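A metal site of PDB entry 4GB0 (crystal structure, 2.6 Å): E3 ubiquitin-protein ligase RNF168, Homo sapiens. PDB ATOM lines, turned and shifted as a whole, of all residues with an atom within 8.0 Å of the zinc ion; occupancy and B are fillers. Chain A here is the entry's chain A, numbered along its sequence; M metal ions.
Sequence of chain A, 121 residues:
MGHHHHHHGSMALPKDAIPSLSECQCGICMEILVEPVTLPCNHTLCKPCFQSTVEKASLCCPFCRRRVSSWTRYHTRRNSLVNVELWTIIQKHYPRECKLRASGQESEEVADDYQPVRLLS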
ATOM      1  N   LEU A  39     -20.466 -10.753   4.236  1.00  0.00           N
ATOM      2  CA  LEU A  39     -19.101 -11.261   4.159  1.00  0.00           C
ATOM      3  C   LEU A  39     -18.358 -10.592   3.012  1.00  0.00           C
ATOM      4  O   LEU A  39     -18.972  -9.883   2.228  1.00  0.00           O
ATOM      5  CB  LEU A  39     -19.116 -12.783   4.044  1.00  0.00           C
ATOM      6  CG  LEU A  39     -19.976 -13.480   5.097  1.00  0.00           C
ATOM      7  CD1 LEU A  39     -20.186 -14.927   4.756  1.00  0.00           C
ATOM      8  CD2 LEU A  39     -19.351 -13.352   6.463  1.00  0.00           C
ATOM      9  N   PRO A  40     -17.020 -10.762   2.931  1.00  0.00           N
ATOM     10  CA  PRO A  40     -16.231 -10.128   1.856  1.00  0.00           C
ATOM     11  C   PRO A  40     -16.577 -10.618   0.463  1.00  0.00           C
ATOM     12  O   PRO A  40     -16.286  -9.928  -0.511  1.00  0.00           O
ATOM     13  CB  PRO A  40     -14.782 -10.474   2.236  1.00  0.00           C
ATOM     14  CG  PRO A  40     -14.872 -11.586   3.199  1.00  0.00           C
ATOM     15  CD  PRO A  40     -16.132 -11.362   3.955  1.00  0.00           C
ATOM     16  N   CYS A  41     -17.210 -11.789   0.376  1.00  0.00           N
ATOM     17  CA  CYS A  41     -17.779 -12.301  -0.879  1.00  0.00           C
ATOM     18  C   CYS A  41     -19.104 -11.639  -1.250  1.00  0.00           C
ATOM     19  O   CYS A  41     -19.627 -11.875  -2.334  1.00  0.00           O
ATOM     20  CB  CYS A  41     -17.999 -13.788  -0.784  1.00  0.00           C
ATOM     21  SG  CYS A  41     -18.839 -14.361   0.725  1.00  0.00           S
ATOM     22  N   ASN A  42     -19.663 -10.856  -0.334  1.00  0.00           N
ATOM     23  CA  ASN A  42     -20.937 -10.150  -0.533  1.00  0.00           C
ATOM     24  C   ASN A  42     -22.194 -10.987  -0.341  1.00  0.00           C
ATOM     25  O   ASN A  42     -23.295 -10.523  -0.637  1.00  0.00           O
ATOM     26  CB  ASN A  42     -20.981  -9.443  -1.886  1.00  0.00           C
ATOM     27  CG  ASN A  42     -20.107  -8.200  -1.911  1.00  0.00           C
ATOM     28  OD1 ASN A  42     -19.258  -8.033  -2.806  1.00  0.00           O
ATOM     29  ND2 ASN A  42     -20.269  -7.328  -0.903  1.00  0.00           N
ATOM     30  N   HIS A  43     -22.025 -12.209   0.153  1.00  0.00           N
ATOM     31  CA  HIS A  43     -23.159 -12.957   0.657  1.00  0.00           C
ATOM     32  C   HIS A  43     -23.473 -12.477   2.072  1.00  0.00           C
ATOM     33  O   HIS A  43     -22.578 -12.102   2.856  1.00  0.00           O
ATOM     34  CB  HIS A  43     -22.885 -14.453   0.604  1.00  0.00           C
ATOM     35  CG  HIS A  43     -22.689 -14.963  -0.783  1.00  0.00           C
ATOM     36  ND1 HIS A  43     -21.442 -15.334  -1.273  1.00  0.00           N
ATOM     37  CD2 HIS A  43     -23.562 -15.106  -1.822  1.00  0.00           C
ATOM     38  CE1 HIS A  43     -21.562 -15.706  -2.532  1.00  0.00           C
ATOM     39  NE2 HIS A  43     -22.835 -15.565  -2.898  1.00  0.00           N
ATOM     40  N   THR A  44     -24.750 -12.471   2.384  1.00  0.00           N
ATOM     41  CA  THR A  44     -25.227 -11.948   3.637  1.00  0.00           C
ATOM     42  C   THR A  44     -25.995 -13.028   4.365  1.00  0.00           C
ATOM     43  O   THR A  44     -26.571 -13.921   3.741  1.00  0.00           O
ATOM     44  CB  THR A  44     -26.090 -10.717   3.386  1.00  0.00           C
ATOM     45  OG1 THR A  44     -25.264  -9.683   2.853  1.00  0.00           O
ATOM     46  CG2 THR A  44     -26.698 -10.208   4.688  1.00  0.00           C
ATOM     47  N   CYS A  60     -16.126 -20.508   6.978  1.00  0.00           N
ATOM     48  CA  CYS A  60     -16.410 -20.437   5.547  1.00  0.00           C
ATOM     49  C   CYS A  60     -17.649 -19.586   5.376  1.00  0.00           C
ATOM     50  O   CYS A  60     -18.446 -19.499   6.282  1.00  0.00           O
ATOM     51  CB  CYS A  60     -16.830 -21.808   5.045  1.00  0.00           C
ATOM     52  SG  CYS A  60     -15.548 -22.912   4.731  1.00  0.00           S
ATOM     53  N   CYS A  61     -17.825 -18.996   4.200  1.00  0.00           N
ATOM     54  CA  CYS A  61     -19.123 -18.537   3.806  1.00  0.00           C
ATOM     55  C   CYS A  61     -19.941 -19.791   3.512  1.00  0.00           C
ATOM     56  O   CYS A  61     -19.448 -20.697   2.870  1.00  0.00           O
ATOM     57  CB  CYS A  61     -19.051 -17.647   2.572  1.00  0.00           C
ATOM     58  SG  CYS A  61     -20.686 -17.238   1.909  1.00  0.00           S
ATOM     59  N   PRO A  62     -21.205 -19.855   3.991  1.00  0.00           N
ATOM     60  CA  PRO A  62     -22.054 -21.045   3.760  1.00  0.00           C
ATOM     61  C   PRO A  62     -22.645 -21.075   2.364  1.00  0.00           C
ATOM     62  O   PRO A  62     -23.178 -22.097   1.937  1.00  0.00           O
ATOM     63  CB  PRO A  62     -23.153 -20.909   4.811  1.00  0.00           C
ATOM     64  CG  PRO A  62     -22.797 -19.722   5.656  1.00  0.00           C
ATOM     65  CD  PRO A  62     -21.867 -18.863   4.860  1.00  0.00           C
ATOM     66  N   PHE A  63     -22.555 -19.970   1.646  1.00  0.00           N
ATOM     67  CA  PHE A  63     -23.024 -19.939   0.263  1.00  0.00           C
ATOM     68  C   PHE A  63     -21.952 -20.356  -0.722  1.00  0.00           C
ATOM     69  O   PHE A  63     -22.238 -21.079  -1.676  1.00  0.00           O
ATOM     70  CB  PHE A  63     -23.542 -18.563  -0.099  1.00  0.00           C
ATOM     71  CG  PHE A  63     -24.672 -18.101   0.765  1.00  0.00           C
ATOM     72  CD1 PHE A  63     -25.966 -18.552   0.523  1.00  0.00           C
ATOM     73  CD2 PHE A  63     -24.444 -17.233   1.834  1.00  0.00           C
ATOM     74  CE1 PHE A  63     -27.030 -18.143   1.328  1.00  0.00           C
ATOM     75  CE2 PHE A  63     -25.486 -16.805   2.644  1.00  0.00           C
ATOM     76  CZ  PHE A  63     -26.796 -17.265   2.389  1.00  0.00           C
ATOM     77  N   CYS A  64     -20.721 -19.909  -0.500  1.00  0.00           N
ATOM     78  CA  CYS A  64     -19.678 -20.013  -1.522  1.00  0.00           C
ATOM     79  C   CYS A  64     -18.353 -20.607  -1.042  1.00  0.00           C
ATOM     80  O   CYS A  64     -17.455 -20.861  -1.851  1.00  0.00           O
ATOM     81  CB  CYS A  64     -19.427 -18.662  -2.184  1.00  0.00           C
ATOM     82  SG  CYS A  64     -18.402 -17.590  -1.189  1.00  0.00           S
ATOM     83  N   ARG A  65     -18.240 -20.829   0.275  1.00  0.00           N
ATOM     84  CA  ARG A  65     -17.099 -21.514   0.892  1.00  0.00           C
ATOM     85  C   ARG A  65     -15.851 -20.617   1.106  1.00  0.00           C
ATOM     86  O   ARG A  65     -14.864 -21.076   1.614  1.00  0.00           O
ATOM     87  CB  ARG A  65     -16.754 -22.795   0.150  1.00  0.00           C
ATOM     88  CG  ARG A  65     -17.898 -23.792   0.080  1.00  0.00           C
ATOM     89  CD  ARG A  65     -18.026 -24.544   1.383  1.00  0.00           C
ATOM     90  NE  ARG A  65     -19.386 -24.476   1.865  1.00  0.00           N
ATOM     91  CZ  ARG A  65     -19.762 -24.637   3.131  1.00  0.00           C
ATOM     92  NH1 ARG A  65     -18.855 -24.893   4.083  1.00  0.00           N
ATOM     93  NH2 ARG A  65     -21.057 -24.547   3.443  1.00  0.00           N
ATOM     94  N   ARG A  66     -15.933 -19.361   0.715  1.00  0.00           N
ATOM     95  CA  ARG A  66     -14.902 -18.381   0.997  1.00  0.00           C
ATOM     96  C   ARG A  66     -14.433 -18.450   2.448  1.00  0.00           C
ATOM     97  O   ARG A  66     -15.251 -18.405   3.374  1.00  0.00           O
ATOM     98  CB  ARG A  66     -15.471 -17.005   0.668  1.00  0.00           C
ATOM     99  CG  ARG A  66     -14.660 -15.814   1.107  1.00  0.00           C
ATOM    100  CD  ARG A  66     -13.840 -15.257  -0.011  1.00  0.00           C
ATOM    101  NE  ARG A  66     -12.986 -14.178   0.483  1.00  0.00           N
ATOM    102  CZ  ARG A  66     -12.976 -12.948  -0.027  1.00  0.00           C
ATOM    103  NH1 ARG A  66     -13.785 -12.661  -1.072  1.00  0.00           N
ATOM    104  NH2 ARG A  66     -12.157 -12.015   0.487  1.00  0.00           N
ATOM    105  N   ARG A  67     -13.120 -18.580   2.659  1.00  0.00           N
ATOM    106  CA  ARG A  67     -12.529 -18.584   4.001  1.00  0.00           C
ATOM    107  C   ARG A  67     -12.708 -17.213   4.590  1.00  0.00           C
ATOM    108  O   ARG A  67     -12.550 -16.220   3.881  1.00  0.00           O
ATOM    109  CB  ARG A  67     -11.056 -18.980   3.988  1.00  0.00           C
ATOM    110  CG  ARG A  67     -10.398 -18.955   5.384  1.00  0.00           C
ATOM    111  CD  ARG A  67      -8.915 -19.216   5.366  1.00  0.00           C
ATOM    112  NE  ARG A  67      -8.193 -18.446   6.394  1.00  0.00           N
ATOM    113  CZ  ARG A  67      -7.261 -17.516   6.152  1.00  0.00           C
ATOM    114  NH1 ARG A  67      -6.698 -16.859   7.174  1.00  0.00           N
ATOM    115  NH2 ARG A  67      -6.896 -17.213   4.910  1.00  0.00           N
ATOM    116  N   VAL A  68     -13.061 -17.149   5.871  1.00  0.00           N
ATOM    117  CA  VAL A  68     -13.488 -15.868   6.429  1.00  0.00           C
ATOM    118  C   VAL A  68     -12.970 -15.637   7.868  1.00  0.00           C
ATOM    119  O   VAL A  68     -13.266 -14.624   8.504  1.00  0.00           O
ATOM    120  CB  VAL A  68     -15.035 -15.713   6.240  1.00  0.00           C
ATOM    121  CG1 VAL A  68     -15.793 -16.018   7.487  1.00  0.00           C
ATOM    122  CG2 VAL A  68     -15.353 -14.370   5.730  1.00  0.00           C
HETATM  123 ZN    ZN M   1     -19.899 -16.170   0.045  1.00  0.00          ZN
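The side-chain sulfur (SG) of Cys 61 lies close to the backbone NH (N) of Phe 63 (3.3 Å).
The backbone NH (N) of Cys 61 sits at hydrogen-bond distance from the backbone carbonyl oxygen (O) of Arg 66, at 2.8 Å.
The backbone NH of Arg 66 lies close to the side-chain sulfur of Cys 64 (3.6 Å).
The zinc ion is bound by ND1 of His 43 (2.2 Å), SG of Cys 41 (2.2 Å), SG of Cys 61 (2.3 Å) and SG of Cys 64 (2.4 Å).
The zinc ion has four donor atoms within binding distance.
Four residues have an atom within 4 Å of the zinc ion: Cys 41, His 43, Cys 61 and Cys 64.
Along chain A the residues within 4 Å of the zinc ion span positions 41 to 64.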
